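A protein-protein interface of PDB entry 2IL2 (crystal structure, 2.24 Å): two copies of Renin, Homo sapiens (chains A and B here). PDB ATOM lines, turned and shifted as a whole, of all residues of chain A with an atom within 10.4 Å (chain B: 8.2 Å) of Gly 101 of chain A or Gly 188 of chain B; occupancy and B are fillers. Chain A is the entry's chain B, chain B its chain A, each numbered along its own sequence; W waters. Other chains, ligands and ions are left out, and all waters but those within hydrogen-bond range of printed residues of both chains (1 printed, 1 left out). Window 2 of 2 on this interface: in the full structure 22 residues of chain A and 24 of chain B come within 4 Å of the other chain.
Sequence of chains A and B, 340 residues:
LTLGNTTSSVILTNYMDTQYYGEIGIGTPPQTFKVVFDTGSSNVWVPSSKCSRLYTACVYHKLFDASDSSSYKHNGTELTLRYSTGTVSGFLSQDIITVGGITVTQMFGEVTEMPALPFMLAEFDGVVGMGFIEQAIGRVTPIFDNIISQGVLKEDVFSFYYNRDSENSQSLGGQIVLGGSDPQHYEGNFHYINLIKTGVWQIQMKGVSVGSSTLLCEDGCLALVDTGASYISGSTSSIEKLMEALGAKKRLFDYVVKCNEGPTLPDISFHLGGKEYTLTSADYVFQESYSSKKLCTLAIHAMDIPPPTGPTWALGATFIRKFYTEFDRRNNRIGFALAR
The side-chain carboxylate (OE1) of Glu 187 of chain B is in hydrogen-bond range of the backbone NH (N) of Ser 9 of chain A. OG1 of Thr 7 of chain A is in hydrogen-bond range of NH1 of Arg 340 of chain B, 3.2 Å away.
NE of Arg 340 of chain B sits at hydrogen-bond distance from O of Tyr 186 of chain B (3.1 Å). The backbone NH of Glu 187 of chain B sits at hydrogen-bond distance from the backbone carbonyl oxygen of Leu 338 of chain B (3.0 Å). The side-chain carboxylate (OE1) of Glu 187 of chain B lies within salt-bridge range of the guanidinium group (NH1) of Arg 340 of chain B, at 3.5 Å. OG of Ser 8 of chain A is in hydrogen-bond range of O of Val 99 of chain A. The backbone carbonyl oxygen (O) of Gly 100 of chain A sits at hydrogen-bond distance from the side-chain hydroxyl (OG) of Ser 8 of chain A, at 2.7 Å. N of Leu 178 of chain A is in hydrogen-bond range of O of Ser 8 of chain A (2.7 Å).
OE1 of Glu 187 of chain B touches CA of Ser 8 of chain A, 3.5 Å away. CB of Arg 340 of chain B touches OG of Ser 9 of chain A (3.4 Å). OE2 of Glu 187 of chain B touches CA of Gly 100 of chain A, at 3.3 Å. Leu 338 of chain B touches Gly 100 of chain A. Gly 101 of chain A touches Gly 188 of chain B.
Printed residues of chain B within 4 Å of Gly 101 of chain A: Gly 188 (3.996 Å). Of the printed residues of chain A, Gly 188 of chain B touches Gly 101. Of the printed residues of chain A, Leu 338 of chain B touches Gly 100 (3.9 Å). Of the printed residues of chain B, Ser 9 of chain A touches Glu 187 and Arg 340. Of the printed residues of chain B, Thr 7 of chain A touches Arg 340 (3.2 Å). Printed residues of chain B within 4 Å of Ser 8 of chain A: Glu 187. Of the printed residues of chain A, Arg 340 of chain B touches Thr 7 and Ser 9. Pro 30 of chain A touches none of the printed residues of chain B. Ile 102 of chain A touches none of the printed residues of chain B. The nearest printed residue of chain A that does not touch Leu 338 of chain B is Gly 101 of chain A (4.4 Å).
Of the 12 printed residues of chain B, 4 touch a printed residue of chain A. Hydrophobic or aromatic side chains of chain B that line the printed part of chain A: Leu 338. Of the 26 printed residues of chain A, 5 touch a printed residue of chain B. Printed residues of chain A that touch a printed residue of chain B: Thr 7, Ser 8, Ser 9, Gly 100 and Gly 101. Along chain A the printed residues that touch a printed residue of chain B span positions 7 to 101. Among the printed residues, 7 pairs touch across the chains. Among the printed residues, no Asp or Glu carboxylate lies within 4 Å of a Lys or Arg side-chain nitrogen of the other chain.
No position is printed for both chains.
Water W1 bridges the guanidinium group of Arg 340 of chain B and the backbone NH of Thr 7 of chain A.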
ATOM      1  N   THR A   6      11.442   8.435 -26.011  1.00  0.00           N
ATOM      2  CA  THR A   6      10.098   8.316 -25.446  1.00  0.00           C
ATOM      3  C   THR A   6       9.209   9.550 -25.653  1.00  0.00           C
ATOM      4  O   THR A   6       9.667  10.663 -25.941  1.00  0.00           O
ATOM      5  CB  THR A   6      10.095   7.976 -23.919  1.00  0.00           C
ATOM      6  OG1 THR A   6      10.394   9.135 -23.139  1.00  0.00           O
ATOM      7  CG2 THR A   6      11.078   6.866 -23.591  1.00  0.00           C
ATOM      8  N   THR A   7       7.911   9.299 -25.532  1.00  0.00           N
ATOM      9  CA  THR A   7       6.913  10.338 -25.419  1.00  0.00           C
ATOM     10  C   THR A   7       6.029   9.982 -24.233  1.00  0.00           C
ATOM     11  O   THR A   7       6.012   8.830 -23.793  1.00  0.00           O
ATOM     12  CB  THR A   7       6.059  10.460 -26.695  1.00  0.00           C
ATOM     13  OG1 THR A   7       5.306   9.249 -26.897  1.00  0.00           O
ATOM     14  CG2 THR A   7       6.963  10.742 -27.921  1.00  0.00           C
ATOM     15  N   SER A   8       5.325  10.980 -23.716  1.00  0.00           N
ATOM     16  CA  SER A   8       4.380  10.792 -22.638  1.00  0.00           C
ATOM     17  C   SER A   8       3.096  11.532 -22.967  1.00  0.00           C
ATOM     18  O   SER A   8       3.108  12.724 -23.250  1.00  0.00           O
ATOM     19  CB  SER A   8       4.959  11.307 -21.332  1.00  0.00           C
ATOM     20  OG  SER A   8       4.147  10.929 -20.244  1.00  0.00           O
ATOM     21  N   SER A   9       1.984  10.824 -22.937  1.00  0.00           N
ATOM     22  CA  SER A   9       0.716  11.456 -23.207  1.00  0.00           C
ATOM     23  C   SER A   9      -0.149  11.502 -21.957  1.00  0.00           C
ATOM     24  O   SER A   9      -0.029  10.669 -21.048  1.00  0.00           O
ATOM     25  CB  SER A   9       0.001  10.745 -24.353  1.00  0.00           C
ATOM     26  OG  SER A   9      -0.332   9.430 -23.986  1.00  0.00           O
ATOM     27  N   VAL A  10      -0.996  12.519 -21.903  1.00  0.00           N
ATOM     28  CA  VAL A  10      -1.942  12.688 -20.814  1.00  0.00           C
ATOM     29  C   VAL A  10      -3.301  13.014 -21.421  1.00  0.00           C
ATOM     30  O   VAL A  10      -3.454  13.996 -22.145  1.00  0.00           O
ATOM     31  CB  VAL A  10      -1.486  13.778 -19.824  1.00  0.00           C
ATOM     32  CG1 VAL A  10      -2.550  13.988 -18.735  1.00  0.00           C
ATOM     33  CG2 VAL A  10      -0.132  13.399 -19.217  1.00  0.00           C
ATOM     34  N   ILE A  11      -4.261  12.155 -21.136  1.00  0.00           N
ATOM     35  CA  ILE A  11      -5.647  12.311 -21.530  1.00  0.00           C
ATOM     36  C   ILE A  11      -6.346  13.400 -20.695  1.00  0.00           C
ATOM     37  O   ILE A  11      -6.203  13.458 -19.458  1.00  0.00           O
ATOM     38  CB  ILE A  11      -6.357  10.936 -21.424  1.00  0.00           C
ATOM     39  CG1 ILE A  11      -5.794  10.021 -22.516  1.00  0.00           C
ATOM     40  CG2 ILE A  11      -7.889  11.069 -21.500  1.00  0.00           C
ATOM     41  CD1 ILE A  11      -6.195   8.553 -22.409  1.00  0.00           C
ATOM     42  N   GLU A  23      -4.731  14.433 -15.309  1.00  0.00           N
ATOM     43  CA  GLU A  23      -4.135  14.005 -14.044  1.00  0.00           C
ATOM     44  C   GLU A  23      -2.619  14.190 -14.001  1.00  0.00           C
ATOM     45  O   GLU A  23      -1.905  13.888 -14.950  1.00  0.00           O
ATOM     46  CB  GLU A  23      -4.455  12.528 -13.764  1.00  0.00           C
ATOM     47  CG  GLU A  23      -5.946  12.173 -13.755  1.00  0.00           C
ATOM     48  CD  GLU A  23      -6.225  10.661 -13.607  1.00  0.00           C
ATOM     49  OE1 GLU A  23      -5.587  10.005 -12.749  1.00  0.00           O
ATOM     50  OE2 GLU A  23      -7.109  10.134 -14.338  1.00  0.00           O
ATOM     51  N   ILE A  24      -2.139  14.701 -12.875  1.00  0.00           N
ATOM     52  CA  ILE A  24      -0.760  14.471 -12.411  1.00  0.00           C
ATOM     53  C   ILE A  24      -0.809  13.864 -11.006  1.00  0.00           C
ATOM     54  O   ILE A  24      -1.764  14.070 -10.253  1.00  0.00           O
ATOM     55  CB  ILE A  24       0.136  15.760 -12.341  1.00  0.00           C
ATOM     56  CG1 ILE A  24      -0.487  16.838 -11.439  1.00  0.00           C
ATOM     57  CG2 ILE A  24       0.430  16.288 -13.711  1.00  0.00           C
ATOM     58  CD1 ILE A  24       0.403  18.021 -11.201  1.00  0.00           C
ATOM     59  N   GLY A  25       0.231  13.115 -10.662  1.00  0.00           N
ATOM     60  CA  GLY A  25       0.403  12.638  -9.287  1.00  0.00           C
ATOM     61  C   GLY A  25       1.538  13.410  -8.656  1.00  0.00           C
ATOM     62  O   GLY A  25       2.531  13.651  -9.312  1.00  0.00           O
ATOM     63  N   PRO A  30       1.933   8.788  -4.813  1.00  0.00           N
ATOM     64  CA  PRO A  30       1.322   9.902  -5.555  1.00  0.00           C
ATOM     65  C   PRO A  30      -0.073  10.338  -5.080  1.00  0.00           C
ATOM     66  O   PRO A  30      -0.979   9.510  -4.975  1.00  0.00           O
ATOM     67  CB  PRO A  30       1.269   9.390  -7.001  1.00  0.00           C
ATOM     68  CG  PRO A  30       1.463   7.904  -6.916  1.00  0.00           C
ATOM     69  CD  PRO A  30       2.218   7.621  -5.669  1.00  0.00           C
ATOM     70  N   PHE A  37      -3.014  22.298 -18.235  1.00  0.00           N
ATOM     71  CA  PHE A  37      -1.691  22.416 -18.814  1.00  0.00           C
ATOM     72  C   PHE A  37      -1.686  23.699 -19.636  1.00  0.00           C
ATOM     73  O   PHE A  37      -2.337  23.784 -20.662  1.00  0.00           O
ATOM     74  CB  PHE A  37      -1.356  21.181 -19.670  1.00  0.00           C
ATOM     75  CG  PHE A  37      -1.251  19.895 -18.868  1.00  0.00           C
ATOM     76  CD1 PHE A  37      -2.385  19.104 -18.617  1.00  0.00           C
ATOM     77  CD2 PHE A  37      -0.029  19.480 -18.363  1.00  0.00           C
ATOM     78  CE1 PHE A  37      -2.291  17.919 -17.886  1.00  0.00           C
ATOM     79  CE2 PHE A  37       0.074  18.290 -17.618  1.00  0.00           C
ATOM     80  CZ  PHE A  37      -1.049  17.512 -17.378  1.00  0.00           C
ATOM     81  N   ILE A  96       8.181  14.714  -6.111  1.00  0.00           N
ATOM     82  CA  ILE A  96       8.141  13.985  -7.373  1.00  0.00           C
ATOM     83  C   ILE A  96       6.738  14.105  -7.996  1.00  0.00           C
ATOM     84  O   ILE A  96       5.734  13.864  -7.327  1.00  0.00           O
ATOM     85  CB  ILE A  96       8.564  12.507  -7.154  1.00  0.00           C
ATOM     86  CG1 ILE A  96      10.005  12.466  -6.609  1.00  0.00           C
ATOM     87  CG2 ILE A  96       8.468  11.715  -8.447  1.00  0.00           C
ATOM     88  CD1 ILE A  96      10.570  11.065  -6.364  1.00  0.00           C
ATOM     89  N   ILE A  97       6.687  14.512  -9.269  1.00  0.00           N
ATOM     90  CA  ILE A  97       5.430  14.672 -10.011  1.00  0.00           C
ATOM     91  C   ILE A  97       5.408  13.679 -11.164  1.00  0.00           C
ATOM     92  O   ILE A  97       6.370  13.579 -11.937  1.00  0.00           O
ATOM     93  CB  ILE A  97       5.238  16.125 -10.539  1.00  0.00           C
ATOM     94  CG1 ILE A  97       5.313  17.128  -9.387  1.00  0.00           C
ATOM     95  CG2 ILE A  97       3.893  16.284 -11.236  1.00  0.00           C
ATOM     96  CD1 ILE A  97       4.870  18.536  -9.752  1.00  0.00           C
ATOM     97  N   THR A  98       4.322  12.926 -11.267  1.00  0.00           N
ATOM     98  CA  THR A  98       4.171  11.966 -12.348  1.00  0.00           C
ATOM     99  C   THR A  98       3.191  12.543 -13.377  1.00  0.00           C
ATOM    100  O   THR A  98       2.068  12.921 -13.030  1.00  0.00           O
ATOM    101  CB  THR A  98       3.739  10.567 -11.832  1.00  0.00           C
ATOM    102  OG1 THR A  98       2.413  10.627 -11.294  1.00  0.00           O
ATOM    103  CG2 THR A  98       4.658  10.102 -10.723  1.00  0.00           C
ATOM    104  N   VAL A  99       3.665  12.656 -14.621  1.00  0.00           N
ATOM    105  CA  VAL A  99       2.893  13.131 -15.758  1.00  0.00           C
ATOM    106  C   VAL A  99       2.948  12.032 -16.834  1.00  0.00           C
ATOM    107  O   VAL A  99       3.999  11.822 -17.451  1.00  0.00           O
ATOM    108  CB  VAL A  99       3.503  14.437 -16.340  1.00  0.00           C
ATOM    109  CG1 VAL A  99       2.485  15.186 -17.174  1.00  0.00           C
ATOM    110  CG2 VAL A  99       4.041  15.327 -15.223  1.00  0.00           C
ATOM    111  N   GLY A 100       1.828  11.334 -17.045  1.00  0.00           N
ATOM    112  CA  GLY A 100       1.787  10.145 -17.899  1.00  0.00           C
ATOM    113  C   GLY A 100       2.946   9.172 -17.693  1.00  0.00           C
ATOM    114  O   GLY A 100       3.645   8.810 -18.622  1.00  0.00           O
ATOM    115  N   GLY A 101       3.199   8.763 -16.475  1.00  0.00           N
ATOM    116  CA  GLY A 101       4.376   7.878 -16.238  1.00  0.00           C
ATOM    117  C   GLY A 101       5.771   8.365 -16.695  1.00  0.00           C
ATOM    118  O   GLY A 101       6.659   7.547 -16.945  1.00  0.00           O
ATOM    119  N   ILE A 102       5.949   9.682 -16.842  1.00  0.00           N
ATOM    120  CA  ILE A 102       7.241  10.324 -16.628  1.00  0.00           C
ATOM    121  C   ILE A 102       7.242  10.788 -15.165  1.00  0.00           C
ATOM    122  O   ILE A 102       6.270  11.382 -14.696  1.00  0.00           O
ATOM    123  CB  ILE A 102       7.467  11.538 -17.565  1.00  0.00           C
ATOM    124  CG1 ILE A 102       7.904  11.070 -18.961  1.00  0.00           C
ATOM    125  CG2 ILE A 102       8.511  12.493 -16.979  1.00  0.00           C
ATOM    126  CD1 ILE A 102       8.069  12.211 -19.982  1.00  0.00           C
ATOM    127  N   THR A 103       8.313  10.482 -14.438  1.00  0.00           N
ATOM    128  CA  THR A 103       8.494  10.959 -13.061  1.00  0.00           C
ATOM    129  C   THR A 103       9.619  12.014 -13.013  1.00  0.00           C
ATOM    130  O   THR A 103      10.712  11.785 -13.530  1.00  0.00           O
ATOM    131  CB  THR A 103       8.803   9.793 -12.118  1.00  0.00           C
ATOM    132  OG1 THR A 103       7.573   9.266 -11.586  1.00  0.00           O
ATOM    133  CG2 THR A 103       9.664  10.242 -10.974  1.00  0.00           C
ATOM    134  N   VAL A 104       9.330  13.169 -12.411  1.00  0.00           N
ATOM    135  CA  VAL A 104      10.251  14.305 -12.409  1.00  0.00           C
ATOM    136  C   VAL A 104      10.184  15.057 -11.072  1.00  0.00           C
ATOM    137  O   VAL A 104       9.100  15.368 -10.576  1.00  0.00           O
ATOM    138  CB  VAL A 104       9.984  15.283 -13.612  1.00  0.00           C
ATOM    139  CG1 VAL A 104       8.581  15.881 -13.558  1.00  0.00           C
ATOM    140  CG2 VAL A 104      11.031  16.396 -13.666  1.00  0.00           C
ATOM    141  N   ILE A 147      12.039  18.183 -17.386  1.00  0.00           N
ATOM    142  CA  ILE A 147      11.839  16.929 -18.134  1.00  0.00           C
ATOM    143  C   ILE A 147      12.813  16.860 -19.312  1.00  0.00           C
ATOM    144  O   ILE A 147      13.327  15.799 -19.607  1.00  0.00           O
ATOM    145  CB  ILE A 147      10.370  16.752 -18.629  1.00  0.00           C
ATOM    146  CG1 ILE A 147       9.431  16.465 -17.457  1.00  0.00           C
ATOM    147  CG2 ILE A 147      10.266  15.631 -19.674  1.00  0.00           C
ATOM    148  CD1 ILE A 147       7.951  16.638 -17.795  1.00  0.00           C
ATOM    149  N   GLN A 150      16.154  15.496 -18.283  1.00  0.00           N
ATOM    150  CA  GLN A 150      16.270  14.057 -18.101  1.00  0.00           C
ATOM    151  C   GLN A 150      16.836  13.371 -19.337  1.00  0.00           C
ATOM    152  O   GLN A 150      17.416  12.281 -19.231  1.00  0.00           O
ATOM    153  CB  GLN A 150      14.919  13.436 -17.766  1.00  0.00           C
ATOM    154  CG  GLN A 150      14.441  13.633 -16.345  1.00  0.00           C
ATOM    155  CD  GLN A 150      13.078  12.995 -16.096  1.00  0.00           C
ATOM    156  OE1 GLN A 150      12.395  12.587 -17.030  1.00  0.00           O
ATOM    157  NE2 GLN A 150      12.674  12.916 -14.830  1.00  0.00           N
ATOM    158  N   VAL A 152      15.169  12.083 -21.932  1.00  0.00           N
ATOM    159  CA  VAL A 152      14.376  10.893 -22.263  1.00  0.00           C
ATOM    160  C   VAL A 152      13.421  11.139 -23.446  1.00  0.00           C
ATOM    161  O   VAL A 152      13.032  10.197 -24.122  1.00  0.00           O
ATOM    162  CB  VAL A 152      13.580  10.373 -21.016  1.00  0.00           C
ATOM    163  CG1 VAL A 152      14.549   9.857 -19.919  1.00  0.00           C
ATOM    164  CG2 VAL A 152      12.633  11.454 -20.465  1.00  0.00           C
ATOM    165  N   LEU A 153      13.075  12.401 -23.706  1.00  0.00           N
ATOM    166  CA  LEU A 153      12.052  12.743 -24.718  1.00  0.00           C
ATOM    167  C   LEU A 153      12.597  12.683 -26.138  1.00  0.00           C
ATOM    168  O   LEU A 153      13.701  13.129 -26.400  1.00  0.00           O
ATOM    169  CB  LEU A 153      11.463  14.140 -24.468  1.00  0.00           C
ATOM    170  CG  LEU A 153      10.570  14.381 -23.244  1.00  0.00           C
ATOM    171  CD1 LEU A 153       9.938  15.775 -23.381  1.00  0.00           C
ATOM    172  CD2 LEU A 153       9.479  13.305 -23.037  1.00  0.00           C
ATOM    173  N   ILE A 176      -2.555  15.849 -24.265  1.00  0.00           N
ATOM    174  CA  ILE A 176      -1.252  16.501 -24.389  1.00  0.00           C
ATOM    175  C   ILE A 176      -0.229  15.390 -24.582  1.00  0.00           C
ATOM    176  O   ILE A 176      -0.323  14.359 -23.922  1.00  0.00           O
ATOM    177  CB  ILE A 176      -0.916  17.449 -23.193  1.00  0.00           C
ATOM    178  CG1 ILE A 176       0.491  18.044 -23.340  1.00  0.00           C
ATOM    179  CG2 ILE A 176      -1.034  16.760 -21.844  1.00  0.00           C
ATOM    180  CD1 ILE A 176       0.896  18.932 -22.144  1.00  0.00           C
ATOM    181  N   LEU A 178       3.854  15.010 -24.496  1.00  0.00           N
ATOM    182  CA  LEU A 178       5.200  15.518 -24.240  1.00  0.00           C
ATOM    183  C   LEU A 178       6.185  14.700 -25.051  1.00  0.00           C
ATOM    184  O   LEU A 178       6.192  13.473 -24.963  1.00  0.00           O
ATOM    185  CB  LEU A 178       5.578  15.390 -22.768  1.00  0.00           C
ATOM    186  CG  LEU A 178       4.523  15.763 -21.722  1.00  0.00           C
ATOM    187  CD1 LEU A 178       5.144  15.606 -20.371  1.00  0.00           C
ATOM    188  CD2 LEU A 178       4.039  17.171 -21.897  1.00  0.00           C
ATOM    189  N   PRO B 183       3.269  -1.872 -26.791  1.00  0.00           N
ATOM    190  CA  PRO B 183       3.805  -0.661 -26.156  1.00  0.00           C
ATOM    191  C   PRO B 183       3.192   0.643 -26.684  1.00  0.00           C
ATOM    192  O   PRO B 183       3.285   1.674 -26.027  1.00  0.00           O
ATOM    193  CB  PRO B 183       5.318  -0.731 -26.451  1.00  0.00           C
ATOM    194  CG  PRO B 183       5.449  -1.665 -27.621  1.00  0.00           C
ATOM    195  CD  PRO B 183       4.323  -2.649 -27.475  1.00  0.00           C
ATOM    196  N   TYR B 186       0.260   1.626 -24.025  1.00  0.00           N
ATOM    197  CA  TYR B 186       0.545   1.864 -22.609  1.00  0.00           C
ATOM    198  C   TYR B 186       1.826   2.695 -22.487  1.00  0.00           C
ATOM    199  O   TYR B 186       2.624   2.774 -23.430  1.00  0.00           O
ATOM    200  CB  TYR B 186       0.648   0.550 -21.818  1.00  0.00           C
ATOM    201  CG  TYR B 186       1.846  -0.339 -22.124  1.00  0.00           C
ATOM    202  CD1 TYR B 186       1.775  -1.336 -23.100  1.00  0.00           C
ATOM    203  CD2 TYR B 186       3.037  -0.214 -21.405  1.00  0.00           C
ATOM    204  CE1 TYR B 186       2.850  -2.159 -23.362  1.00  0.00           C
ATOM    205  CE2 TYR B 186       4.120  -1.026 -21.665  1.00  0.00           C
ATOM    206  CZ  TYR B 186       4.028  -1.991 -22.647  1.00  0.00           C
ATOM    207  OH  TYR B 186       5.107  -2.807 -22.904  1.00  0.00           O
ATOM    208  N   GLU B 187       1.984   3.355 -21.343  1.00  0.00           N
ATOM    209  CA  GLU B 187       3.193   4.115 -21.035  1.00  0.00           C
ATOM    210  C   GLU B 187       3.576   3.862 -19.590  1.00  0.00           C
ATOM    211  O   GLU B 187       2.795   3.304 -18.817  1.00  0.00           O
ATOM    212  CB  GLU B 187       3.001   5.616 -21.275  1.00  0.00           C
ATOM    213  CG  GLU B 187       1.753   6.203 -20.629  1.00  0.00           C
ATOM    214  CD  GLU B 187       1.509   7.636 -21.019  1.00  0.00           C
ATOM    215  OE1 GLU B 187       2.166   8.117 -21.962  1.00  0.00           O
ATOM    216  OE2 GLU B 187       0.644   8.269 -20.380  1.00  0.00           O
ATOM    217  N   GLY B 188       4.792   4.270 -19.240  1.00  0.00           N
ATOM    218  CA  GLY B 188       5.396   3.898 -17.973  1.00  0.00           C
ATOM    219  C   GLY B 188       5.596   2.403 -17.949  1.00  0.00           C
ATOM    220  O   GLY B 188       5.609   1.743 -18.999  1.00  0.00           O
ATOM    221  N   ASN B 189       5.731   1.865 -16.745  1.00  0.00           N
ATOM    222  CA  ASN B 189       6.068   0.451 -16.566  1.00  0.00           C
ATOM    223  C   ASN B 189       4.889  -0.344 -16.046  1.00  0.00           C
ATOM    224  O   ASN B 189       4.037   0.184 -15.324  1.00  0.00           O
ATOM    225  CB  ASN B 189       7.241   0.296 -15.593  1.00  0.00           C
ATOM    226  CG  ASN B 189       8.536   0.870 -16.140  1.00  0.00           C
ATOM    227  OD1 ASN B 189       9.236   1.611 -15.442  1.00  0.00           O
ATOM    228  ND2 ASN B 189       8.861   0.538 -17.391  1.00  0.00           N
ATOM    229  N   PHE B 190       4.857  -1.618 -16.421  1.00  0.00           N
ATOM    230  CA  PHE B 190       3.888  -2.540 -15.884  1.00  0.00           C
ATOM    231  C   PHE B 190       4.158  -2.686 -14.400  1.00  0.00           C
ATOM    232  O   PHE B 190       5.304  -2.589 -13.944  1.00  0.00           O
ATOM    233  CB  PHE B 190       3.945  -3.902 -16.586  1.00  0.00           C
ATOM    234  CG  PHE B 190       3.069  -4.002 -17.816  1.00  0.00           C
ATOM    235  CD1 PHE B 190       3.627  -4.070 -19.091  1.00  0.00           C
ATOM    236  CD2 PHE B 190       1.693  -4.059 -17.699  1.00  0.00           C
ATOM    237  CE1 PHE B 190       2.827  -4.173 -20.213  1.00  0.00           C
ATOM    238  CE2 PHE B 190       0.881  -4.160 -18.824  1.00  0.00           C
ATOM    239  CZ  PHE B 190       1.450  -4.219 -20.078  1.00  0.00           C
ATOM    240  N   HIS B 191       3.090  -2.876 -13.641  1.00  0.00           N
ATOM    241  CA  HIS B 191       3.210  -3.276 -12.244  1.00  0.00           C
ATOM    242  C   HIS B 191       2.354  -4.506 -12.062  1.00  0.00           C
ATOM    243  O   HIS B 191       1.216  -4.551 -12.518  1.00  0.00           O
ATOM    244  CB  HIS B 191       2.818  -2.142 -11.304  1.00  0.00           C
ATOM    245  CG  HIS B 191       3.833  -1.044 -11.266  1.00  0.00           C
ATOM    246  ND1 HIS B 191       3.684   0.136 -11.965  1.00  0.00           N
ATOM    247  CD2 HIS B 191       5.048  -0.979 -10.668  1.00  0.00           C
ATOM    248  CE1 HIS B 191       4.748   0.893 -11.769  1.00  0.00           C
ATOM    249  NE2 HIS B 191       5.594   0.237 -10.992  1.00  0.00           N
ATOM    250  N   PHE B 336      -0.521  -4.167 -14.795  1.00  0.00           N
ATOM    251  CA  PHE B 336      -1.224  -2.958 -15.220  1.00  0.00           C
ATOM    252  C   PHE B 336      -0.232  -1.860 -15.617  1.00  0.00           C
ATOM    253  O   PHE B 336       0.829  -1.693 -15.002  1.00  0.00           O
ATOM    254  CB  PHE B 336      -2.115  -2.445 -14.093  1.00  0.00           C
ATOM    255  CG  PHE B 336      -3.248  -3.366 -13.738  1.00  0.00           C
ATOM    256  CD1 PHE B 336      -3.299  -3.981 -12.488  1.00  0.00           C
ATOM    257  CD2 PHE B 336      -4.282  -3.606 -14.643  1.00  0.00           C
ATOM    258  CE1 PHE B 336      -4.351  -4.818 -12.153  1.00  0.00           C
ATOM    259  CE2 PHE B 336      -5.346  -4.448 -14.307  1.00  0.00           C
ATOM    260  CZ  PHE B 336      -5.381  -5.047 -13.069  1.00  0.00           C
ATOM    261  N   ALA B 337      -0.578  -1.124 -16.664  1.00  0.00           N
ATOM    262  CA  ALA B 337       0.134   0.104 -17.003  1.00  0.00           C
ATOM    263  C   ALA B 337      -0.873   1.131 -17.479  1.00  0.00           C
ATOM    264  O   ALA B 337      -1.974   0.774 -17.900  1.00  0.00           O
ATOM    265  CB  ALA B 337       1.236  -0.141 -18.073  1.00  0.00           C
ATOM    266  N   LEU B 338      -0.494   2.398 -17.414  1.00  0.00           N
ATOM    267  CA  LEU B 338      -1.384   3.488 -17.813  1.00  0.00           C
ATOM    268  C   LEU B 338      -1.639   3.403 -19.317  1.00  0.00           C
ATOM    269  O   LEU B 338      -0.721   3.529 -20.101  1.00  0.00           O
ATOM    270  CB  LEU B 338      -0.746   4.844 -17.506  1.00  0.00           C
ATOM    271  CG  LEU B 338      -1.527   6.020 -16.918  1.00  0.00           C
ATOM    272  CD1 LEU B 338      -0.843   7.354 -17.347  1.00  0.00           C
ATOM    273  CD2 LEU B 338      -3.014   6.006 -17.153  1.00  0.00           C
ATOM    274  N   ALA B 339      -2.889   3.235 -19.705  1.00  0.00           N
ATOM    275  CA  ALA B 339      -3.237   3.169 -21.114  1.00  0.00           C
ATOM    276  C   ALA B 339      -3.026   4.513 -21.820  1.00  0.00           C
ATOM    277  O   ALA B 339      -3.192   5.595 -21.219  1.00  0.00           O
ATOM    278  CB  ALA B 339      -4.642   2.707 -21.293  1.00  0.00           C
ATOM    279  N   ARG B 340      -2.636   4.417 -23.096  1.00  0.00           N
ATOM    280  CA  ARG B 340      -2.709   5.547 -24.008  1.00  0.00           C
ATOM    281  C   ARG B 340      -3.202   5.150 -25.417  1.00  0.00           C
ATOM    282  O   ARG B 340      -3.472   6.040 -26.239  1.00  0.00           O
ATOM    283  CB  ARG B 340      -1.346   6.210 -24.111  1.00  0.00           C
ATOM    284  CG  ARG B 340      -0.239   5.270 -24.485  1.00  0.00           C
ATOM    285  CD  ARG B 340       0.822   6.015 -25.217  1.00  0.00           C
ATOM    286  NE  ARG B 340       2.111   5.381 -25.119  1.00  0.00           N
ATOM    287  CZ  ARG B 340       3.267   6.053 -25.127  1.00  0.00           C
ATOM    288  NH1 ARG B 340       3.279   7.391 -25.232  1.00  0.00           N
ATOM    289  NH2 ARG B 340       4.420   5.390 -25.023  1.00  0.00           N
ATOM    290  OXT ARG B 340      -3.324   3.962 -25.788  1.00  0.00           O
HETATM  291  O   HOH W   1       7.402   6.189 -25.514  1.00  0.00           O
